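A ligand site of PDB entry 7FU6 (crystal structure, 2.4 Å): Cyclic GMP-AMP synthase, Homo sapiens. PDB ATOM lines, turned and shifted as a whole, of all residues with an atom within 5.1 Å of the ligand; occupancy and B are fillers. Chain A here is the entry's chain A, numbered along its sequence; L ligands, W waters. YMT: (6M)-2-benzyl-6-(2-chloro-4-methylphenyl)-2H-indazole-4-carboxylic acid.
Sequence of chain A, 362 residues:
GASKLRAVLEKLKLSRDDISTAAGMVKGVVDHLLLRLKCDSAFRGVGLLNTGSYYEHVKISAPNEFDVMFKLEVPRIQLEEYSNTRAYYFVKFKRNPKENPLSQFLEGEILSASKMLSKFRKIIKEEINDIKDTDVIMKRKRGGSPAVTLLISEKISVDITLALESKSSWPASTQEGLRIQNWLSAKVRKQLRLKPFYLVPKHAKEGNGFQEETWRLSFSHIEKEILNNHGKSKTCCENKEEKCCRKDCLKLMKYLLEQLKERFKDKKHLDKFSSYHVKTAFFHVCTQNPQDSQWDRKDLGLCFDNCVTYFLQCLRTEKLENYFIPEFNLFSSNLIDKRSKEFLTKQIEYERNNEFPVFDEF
OG of Ser 218 lies within hydrogen-bond range of O14 of the ligand, at 3.0 Å.
An oxygen (O13) of the ligand sits at hydrogen-bond distance from the backbone NH of Phe 219 (2.9 Å).
O14 of the ligand lies within salt-bridge range of NH1 of Arg 216.
OH of Tyr 323 lies close to O of Phe 283, at 3.4 Å.
The backbone carbonyl oxygen (O) of Tyr 276 is in hydrogen-bond range of the side-chain hydroxyl (OG1) of Thr 280.
The side-chain carboxylate (OE2) of Glu 56 is in salt-bridge range of the side-chain amino group (NZ) of Lys 279, at 3.99 Å.
O of Tyr 323 sits at hydrogen-bond distance from N of Leu 178 (2.8 Å).
NZ of Lys 279 lies within salt-bridge range of OE1 of Glu 223, at 2.8 Å.
ND2 of Asn 322 sits at hydrogen-bond distance from OH of Tyr 276 (3.4 Å).
SD of Met 69 sits at hydrogen-bond distance from OG of Ser 220 (3.7 Å).
The backbone NH (N) of Phe 324 is in hydrogen-bond range of the side-chain amide oxygen (OD1) of Asn 322, at 3.0 Å.
Water W1 lies within hydrogen-bond range of N of Tyr 323, OG1 of Thr 280 and OH of Tyr 276.
Residues that only touch the ligand: Thr 280, Asp 67, Phe 283, Glu 223, Ser 220, Glu 56, Tyr 276, Phe 324, Met 69, Ile 226, Ile 222, Tyr 323 and Lys 279.
Hydrophobic or aromatic side chains that line the ligand: Met 69, Phe 219, Ile 226, Tyr 276, Phe 283, Tyr 323 and Phe 324.
The nearest printed residue that does not touch the ligand is Leu 217 (4.2 Å).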
ATOM      1  N   THR A  51      21.967  27.146 -26.567  1.00  0.00           N
ATOM      2  CA  THR A  51      22.535  28.003 -25.508  1.00  0.00           C
ATOM      3  C   THR A  51      21.651  29.289 -25.442  1.00  0.00           C
ATOM      4  O   THR A  51      21.926  30.244 -24.699  1.00  0.00           O
ATOM      5  CB  THR A  51      24.059  28.279 -25.754  1.00  0.00           C
ATOM      6  OG1 THR A  51      24.331  28.549 -27.133  1.00  0.00           O
ATOM      7  CG2 THR A  51      24.953  27.152 -25.258  1.00  0.00           C
ATOM      8  N   GLU A  56      22.571  33.180 -29.596  1.00  0.00           N
ATOM      9  CA  GLU A  56      23.372  33.202 -28.353  1.00  0.00           C
ATOM     10  C   GLU A  56      24.456  34.273 -28.532  1.00  0.00           C
ATOM     11  O   GLU A  56      25.172  34.280 -29.543  1.00  0.00           O
ATOM     12  CB  GLU A  56      23.936  31.815 -27.983  1.00  0.00           C
ATOM     13  CG  GLU A  56      25.068  31.811 -26.953  1.00  0.00           C
ATOM     14  CD  GLU A  56      24.825  32.233 -25.516  1.00  0.00           C
ATOM     15  OE1 GLU A  56      23.683  32.626 -25.173  1.00  0.00           O
ATOM     16  OE2 GLU A  56      25.788  32.151 -24.712  1.00  0.00           O
ATOM     17  N   ASP A  67      27.639  34.086 -30.755  1.00  0.00           N
ATOM     18  CA  ASP A  67      28.405  32.899 -30.413  1.00  0.00           C
ATOM     19  C   ASP A  67      27.542  31.660 -30.575  1.00  0.00           C
ATOM     20  O   ASP A  67      26.584  31.482 -29.835  1.00  0.00           O
ATOM     21  CB  ASP A  67      28.980  33.016 -28.982  1.00  0.00           C
ATOM     22  CG  ASP A  67      30.431  33.425 -29.003  1.00  0.00           C
ATOM     23  OD1 ASP A  67      30.703  34.646 -29.191  1.00  0.00           O
ATOM     24  OD2 ASP A  67      31.305  32.544 -28.861  1.00  0.00           O
ATOM     25  N   VAL A  68      27.853  30.794 -31.571  1.00  0.00           N
ATOM     26  CA  VAL A  68      27.058  29.577 -31.760  1.00  0.00           C
ATOM     27  C   VAL A  68      27.881  28.334 -31.371  1.00  0.00           C
ATOM     28  O   VAL A  68      29.110  28.316 -31.479  1.00  0.00           O
ATOM     29  CB  VAL A  68      26.313  29.452 -33.134  1.00  0.00           C
ATOM     30  CG1 VAL A  68      25.564  30.728 -33.490  1.00  0.00           C
ATOM     31  CG2 VAL A  68      27.231  29.052 -34.270  1.00  0.00           C
ATOM     32  N   MET A  69      27.198  27.318 -30.859  1.00  0.00           N
ATOM     33  CA  MET A  69      27.802  26.062 -30.442  1.00  0.00           C
ATOM     34  C   MET A  69      27.135  24.880 -31.169  1.00  0.00           C
ATOM     35  O   MET A  69      25.908  24.775 -31.206  1.00  0.00           O
ATOM     36  CB  MET A  69      27.710  25.887 -28.922  1.00  0.00           C
ATOM     37  CG  MET A  69      28.769  24.965 -28.354  1.00  0.00           C
ATOM     38  SD  MET A  69      29.032  25.300 -26.600  1.00  0.00           S
ATOM     39  CE  MET A  69      30.406  26.389 -26.690  1.00  0.00           C
ATOM     40  N   THR A 161      31.815  27.258 -32.253  1.00  0.00           N
ATOM     41  CA  THR A 161      32.568  26.348 -31.398  1.00  0.00           C
ATOM     42  C   THR A 161      31.937  24.973 -31.567  1.00  0.00           C
ATOM     43  O   THR A 161      30.705  24.848 -31.614  1.00  0.00           O
ATOM     44  CB  THR A 161      32.508  26.842 -29.924  1.00  0.00           C
ATOM     45  OG1 THR A 161      32.749  28.253 -29.825  1.00  0.00           O
ATOM     46  CG2 THR A 161      33.447  26.084 -29.011  1.00  0.00           C
ATOM     47  N   LEU A 178      28.653  24.343  -8.960  1.00  0.00           N
ATOM     48  CA  LEU A 178      27.230  24.633  -9.056  1.00  0.00           C
ATOM     49  C   LEU A 178      26.593  24.751  -7.639  1.00  0.00           C
ATOM     50  O   LEU A 178      25.615  24.063  -7.329  1.00  0.00           O
ATOM     51  CB  LEU A 178      26.516  23.596  -9.972  1.00  0.00           C
ATOM     52  CG  LEU A 178      25.085  23.931 -10.506  1.00  0.00           C
ATOM     53  CD1 LEU A 178      25.054  25.261 -11.330  1.00  0.00           C
ATOM     54  CD2 LEU A 178      24.495  22.767 -11.296  1.00  0.00           C
ATOM     55  N   ARG A 216      38.503  21.192 -22.697  1.00  0.00           N
ATOM     56  CA  ARG A 216      37.956  21.643 -21.410  1.00  0.00           C
ATOM     57  C   ARG A 216      36.485  21.449 -21.322  1.00  0.00           C
ATOM     58  O   ARG A 216      35.787  21.569 -22.325  1.00  0.00           O
ATOM     59  CB  ARG A 216      38.345  23.083 -20.971  1.00  0.00           C
ATOM     60  CG  ARG A 216      38.109  24.184 -21.947  1.00  0.00           C
ATOM     61  CD  ARG A 216      37.932  25.532 -21.250  1.00  0.00           C
ATOM     62  NE  ARG A 216      37.218  26.474 -22.118  1.00  0.00           N
ATOM     63  CZ  ARG A 216      35.896  26.658 -22.113  1.00  0.00           C
ATOM     64  NH1 ARG A 216      35.120  25.974 -21.263  1.00  0.00           N
ATOM     65  NH2 ARG A 216      35.329  27.512 -22.960  1.00  0.00           N
ATOM     66  N   LEU A 217      36.027  21.172 -20.086  1.00  0.00           N
ATOM     67  CA  LEU A 217      34.623  21.013 -19.729  1.00  0.00           C
ATOM     68  C   LEU A 217      33.926  22.338 -19.901  1.00  0.00           C
ATOM     69  O   LEU A 217      34.416  23.382 -19.441  1.00  0.00           O
ATOM     70  CB  LEU A 217      34.430  20.579 -18.264  1.00  0.00           C
ATOM     71  CG  LEU A 217      35.169  19.386 -17.723  1.00  0.00           C
ATOM     72  CD1 LEU A 217      34.762  19.161 -16.279  1.00  0.00           C
ATOM     73  CD2 LEU A 217      34.910  18.138 -18.572  1.00  0.00           C
ATOM     74  N   SER A 218      32.753  22.284 -20.529  1.00  0.00           N
ATOM     75  CA  SER A 218      31.881  23.414 -20.814  1.00  0.00           C
ATOM     76  C   SER A 218      30.495  23.073 -20.250  1.00  0.00           C
ATOM     77  O   SER A 218      30.003  21.943 -20.373  1.00  0.00           O
ATOM     78  CB  SER A 218      31.826  23.672 -22.321  1.00  0.00           C
ATOM     79  OG  SER A 218      31.359  24.979 -22.644  1.00  0.00           O
ATOM     80  N   PHE A 219      29.918  24.051 -19.537  1.00  0.00           N
ATOM     81  CA  PHE A 219      28.602  23.990 -18.913  1.00  0.00           C
ATOM     82  C   PHE A 219      27.823  25.228 -19.292  1.00  0.00           C
ATOM     83  O   PHE A 219      26.974  25.676 -18.532  1.00  0.00           O
ATOM     84  CB  PHE A 219      28.758  23.888 -17.392  1.00  0.00           C
ATOM     85  CG  PHE A 219      29.449  22.617 -16.964  1.00  0.00           C
ATOM     86  CD1 PHE A 219      28.747  21.405 -16.908  1.00  0.00           C
ATOM     87  CD2 PHE A 219      30.800  22.608 -16.645  1.00  0.00           C
ATOM     88  CE1 PHE A 219      29.390  20.235 -16.542  1.00  0.00           C
ATOM     89  CE2 PHE A 219      31.437  21.426 -16.240  1.00  0.00           C
ATOM     90  CZ  PHE A 219      30.724  20.245 -16.202  1.00  0.00           C
ATOM     91  N   SER A 220      28.082  25.761 -20.495  1.00  0.00           N
ATOM     92  CA  SER A 220      27.474  26.988 -21.010  1.00  0.00           C
ATOM     93  C   SER A 220      25.925  26.890 -21.207  1.00  0.00           C
ATOM     94  O   SER A 220      25.242  27.895 -21.039  1.00  0.00           O
ATOM     95  CB  SER A 220      28.162  27.462 -22.283  1.00  0.00           C
ATOM     96  OG  SER A 220      27.702  26.759 -23.422  1.00  0.00           O
ATOM     97  N   ILE A 222      23.854  25.519 -19.247  1.00  0.00           N
ATOM     98  CA  ILE A 222      23.215  25.638 -17.929  1.00  0.00           C
ATOM     99  C   ILE A 222      22.788  27.092 -17.605  1.00  0.00           C
ATOM    100  O   ILE A 222      21.878  27.306 -16.779  1.00  0.00           O
ATOM    101  CB  ILE A 222      24.131  25.012 -16.811  1.00  0.00           C
ATOM    102  CG1 ILE A 222      24.446  23.494 -17.073  1.00  0.00           C
ATOM    103  CG2 ILE A 222      23.597  25.260 -15.367  1.00  0.00           C
ATOM    104  CD1 ILE A 222      23.253  22.535 -17.199  1.00  0.00           C
ATOM    105  N   GLU A 223      23.453  28.081 -18.233  1.00  0.00           N
ATOM    106  CA  GLU A 223      23.150  29.505 -18.047  1.00  0.00           C
ATOM    107  C   GLU A 223      21.676  29.853 -18.320  1.00  0.00           C
ATOM    108  O   GLU A 223      21.042  30.462 -17.478  1.00  0.00           O
ATOM    109  CB  GLU A 223      24.042  30.334 -18.939  1.00  0.00           C
ATOM    110  CG  GLU A 223      24.251  31.731 -18.396  1.00  0.00           C
ATOM    111  CD  GLU A 223      24.726  32.735 -19.427  1.00  0.00           C
ATOM    112  OE1 GLU A 223      25.405  32.324 -20.400  1.00  0.00           O
ATOM    113  OE2 GLU A 223      24.438  33.943 -19.239  1.00  0.00           O
ATOM    114  N   ILE A 226      19.167  28.580 -15.655  1.00  0.00           N
ATOM    115  CA  ILE A 226      19.188  29.421 -14.467  1.00  0.00           C
ATOM    116  C   ILE A 226      18.704  30.851 -14.744  1.00  0.00           C
ATOM    117  O   ILE A 226      17.882  31.320 -13.986  1.00  0.00           O
ATOM    118  CB  ILE A 226      20.568  29.366 -13.805  1.00  0.00           C
ATOM    119  CG1 ILE A 226      20.799  27.915 -13.273  1.00  0.00           C
ATOM    120  CG2 ILE A 226      20.661  30.416 -12.700  1.00  0.00           C
ATOM    121  CD1 ILE A 226      22.071  27.596 -12.620  1.00  0.00           C
ATOM    122  N   TYR A 276      32.297  36.084 -20.003  1.00  0.00           N
ATOM    123  CA  TYR A 276      32.398  34.863 -19.220  1.00  0.00           C
ATOM    124  C   TYR A 276      32.930  35.091 -17.792  1.00  0.00           C
ATOM    125  O   TYR A 276      32.429  34.487 -16.859  1.00  0.00           O
ATOM    126  CB  TYR A 276      33.295  33.887 -19.965  1.00  0.00           C
ATOM    127  CG  TYR A 276      33.552  32.625 -19.194  1.00  0.00           C
ATOM    128  CD1 TYR A 276      32.499  31.810 -18.770  1.00  0.00           C
ATOM    129  CD2 TYR A 276      34.857  32.208 -18.917  1.00  0.00           C
ATOM    130  CE1 TYR A 276      32.737  30.630 -18.066  1.00  0.00           C
ATOM    131  CE2 TYR A 276      35.101  31.033 -18.219  1.00  0.00           C
ATOM    132  CZ  TYR A 276      34.032  30.236 -17.815  1.00  0.00           C
ATOM    133  OH  TYR A 276      34.270  29.055 -17.152  1.00  0.00           O
ATOM    134  N   LYS A 279      30.046  36.871 -16.104  1.00  0.00           N
ATOM    135  CA  LYS A 279      28.988  35.885 -15.751  1.00  0.00           C
ATOM    136  C   LYS A 279      29.353  35.105 -14.510  1.00  0.00           C
ATOM    137  O   LYS A 279      28.572  35.107 -13.573  1.00  0.00           O
ATOM    138  CB  LYS A 279      28.708  34.898 -16.900  1.00  0.00           C
ATOM    139  CG  LYS A 279      27.939  35.494 -18.068  1.00  0.00           C
ATOM    140  CD  LYS A 279      28.000  34.567 -19.274  1.00  0.00           C
ATOM    141  CE  LYS A 279      27.369  35.198 -20.487  1.00  0.00           C
ATOM    142  NZ  LYS A 279      27.141  34.200 -21.562  1.00  0.00           N
ATOM    143  N   THR A 280      30.545  34.459 -14.489  1.00  0.00           N
ATOM    144  CA  THR A 280      31.053  33.678 -13.369  1.00  0.00           C
ATOM    145  C   THR A 280      30.984  34.454 -12.073  1.00  0.00           C
ATOM    146  O   THR A 280      30.451  33.930 -11.125  1.00  0.00           O
ATOM    147  CB  THR A 280      32.493  33.194 -13.642  1.00  0.00           C
ATOM    148  OG1 THR A 280      32.462  32.375 -14.796  1.00  0.00           O
ATOM    149  CG2 THR A 280      33.064  32.367 -12.497  1.00  0.00           C
ATOM    150  N   PHE A 283      27.387  35.088 -10.886  1.00  0.00           N
ATOM    151  CA  PHE A 283      26.750  33.894 -10.348  1.00  0.00           C
ATOM    152  C   PHE A 283      27.271  33.552  -8.968  1.00  0.00           C
ATOM    153  O   PHE A 283      26.497  33.018  -8.180  1.00  0.00           O
ATOM    154  CB  PHE A 283      26.802  32.717 -11.339  1.00  0.00           C
ATOM    155  CG  PHE A 283      25.758  32.865 -12.428  1.00  0.00           C
ATOM    156  CD1 PHE A 283      24.392  32.845 -12.118  1.00  0.00           C
ATOM    157  CD2 PHE A 283      26.132  33.068 -13.757  1.00  0.00           C
ATOM    158  CE1 PHE A 283      23.417  32.961 -13.138  1.00  0.00           C
ATOM    159  CE2 PHE A 283      25.161  33.204 -14.768  1.00  0.00           C
ATOM    160  CZ  PHE A 283      23.811  33.122 -14.452  1.00  0.00           C
ATOM    161  N   ASN A 322      35.973  28.822 -11.439  1.00  0.00           N
ATOM    162  CA  ASN A 322      35.030  28.318 -12.412  1.00  0.00           C
ATOM    163  C   ASN A 322      33.823  27.870 -11.566  1.00  0.00           C
ATOM    164  O   ASN A 322      33.998  27.176 -10.545  1.00  0.00           O
ATOM    165  CB  ASN A 322      35.675  27.147 -13.167  1.00  0.00           C
ATOM    166  CG  ASN A 322      34.819  26.518 -14.217  1.00  0.00           C
ATOM    167  OD1 ASN A 322      33.674  26.181 -14.005  1.00  0.00           O
ATOM    168  ND2 ASN A 322      35.383  26.319 -15.383  1.00  0.00           N
ATOM    169  N   TYR A 323      32.623  28.352 -11.934  1.00  0.00           N
ATOM    170  CA  TYR A 323      31.383  28.150 -11.220  1.00  0.00           C
ATOM    171  C   TYR A 323      31.002  26.675 -11.050  1.00  0.00           C
ATOM    172  O   TYR A 323      30.304  26.327 -10.083  1.00  0.00           O
ATOM    173  CB  TYR A 323      30.268  28.955 -11.878  1.00  0.00           C
ATOM    174  CG  TYR A 323      29.087  29.170 -10.974  1.00  0.00           C
ATOM    175  CD1 TYR A 323      29.114  30.124  -9.965  1.00  0.00           C
ATOM    176  CD2 TYR A 323      27.937  28.377 -11.089  1.00  0.00           C
ATOM    177  CE1 TYR A 323      28.048  30.286  -9.080  1.00  0.00           C
ATOM    178  CE2 TYR A 323      26.856  28.541 -10.220  1.00  0.00           C
ATOM    179  CZ  TYR A 323      26.909  29.511  -9.239  1.00  0.00           C
ATOM    180  OH  TYR A 323      25.849  29.725  -8.403  1.00  0.00           O
ATOM    181  N   PHE A 324      31.535  25.808 -11.947  1.00  0.00           N
ATOM    182  CA  PHE A 324      31.306  24.359 -11.993  1.00  0.00           C
ATOM    183  C   PHE A 324      32.494  23.547 -11.473  1.00  0.00           C
ATOM    184  O   PHE A 324      32.318  22.414 -11.078  1.00  0.00           O
ATOM    185  CB  PHE A 324      30.952  23.924 -13.422  1.00  0.00           C
ATOM    186  CG  PHE A 324      29.632  24.501 -13.869  1.00  0.00           C
ATOM    187  CD1 PHE A 324      29.542  25.811 -14.331  1.00  0.00           C
ATOM    188  CD2 PHE A 324      28.456  23.746 -13.772  1.00  0.00           C
ATOM    189  CE1 PHE A 324      28.325  26.366 -14.674  1.00  0.00           C
ATOM    190  CE2 PHE A 324      27.241  24.289 -14.146  1.00  0.00           C
ATOM    191  CZ  PHE A 324      27.172  25.598 -14.561  1.00  0.00           C
HETATM  192  C10 YMT L   1      29.750  28.304 -18.445  1.00  0.00           C
HETATM  193  C11 YMT L   1      30.580  28.249 -19.563  1.00  0.00           C
HETATM  194  O14 YMT L   1      32.297  27.002 -20.614  1.00  0.00           O
HETATM  195  C15 YMT L   1      30.525  29.273 -20.541  1.00  0.00           C
HETATM  196  C16 YMT L   1      29.575  30.309 -20.394  1.00  0.00           C
HETATM  197  C17 YMT L   1      28.756  30.330 -19.241  1.00  0.00           C
HETATM  198  C20 YMT L   1      31.169  29.544 -21.789  1.00  0.00           C
HETATM  199  C21 YMT L   1      30.974  31.331 -23.542  1.00  0.00           C
HETATM  200  C22 YMT L   1      30.224  30.765 -24.725  1.00  0.00           C
HETATM  201  C23 YMT L   1      28.888  30.353 -24.603  1.00  0.00           C
HETATM  202  C24 YMT L   1      28.206  29.819 -25.683  1.00  0.00           C
HETATM  203  C25 YMT L   1      28.839  29.685 -26.903  1.00  0.00           C
HETATM  204  C26 YMT L   1      30.163  30.082 -27.039  1.00  0.00           C
HETATM  205  C27 YMT L   1      30.843  30.633 -25.963  1.00  0.00           C
HETATM  206  C1  YMT L   1      25.217  29.382 -13.686  1.00  0.00           C
HETATM  207  C2  YMT L   1      26.160  29.391 -14.866  1.00  0.00           C
HETATM  208  C3  YMT L   1      27.313  30.161 -14.855  1.00  0.00           C
HETATM  209  C4  YMT L   1      28.181  30.146 -15.937  1.00  0.00           C
HETATM  210 CL5  YMT L   1      29.639  31.094 -15.809  1.00  0.00          CL
HETATM  211  C6  YMT L   1      27.938  29.366 -17.073  1.00  0.00           C
HETATM  212  C7  YMT L   1      26.770  28.602 -17.077  1.00  0.00           C
HETATM  213  C8  YMT L   1      25.908  28.622 -15.999  1.00  0.00           C
HETATM  214  C9  YMT L   1      28.828  29.337 -18.264  1.00  0.00           C
HETATM  215  C12 YMT L   1      31.550  27.118 -19.657  1.00  0.00           C
HETATM  216  O13 YMT L   1      31.568  26.320 -18.638  1.00  0.00           O
HETATM  217  N18 YMT L   1      29.659  31.203 -21.451  1.00  0.00           N
HETATM  218  N19 YMT L   1      30.618  30.672 -22.271  1.00  0.00           N
HETATM  219  O   HOH W   1      32.418  29.440 -14.591  1.00  0.00           O
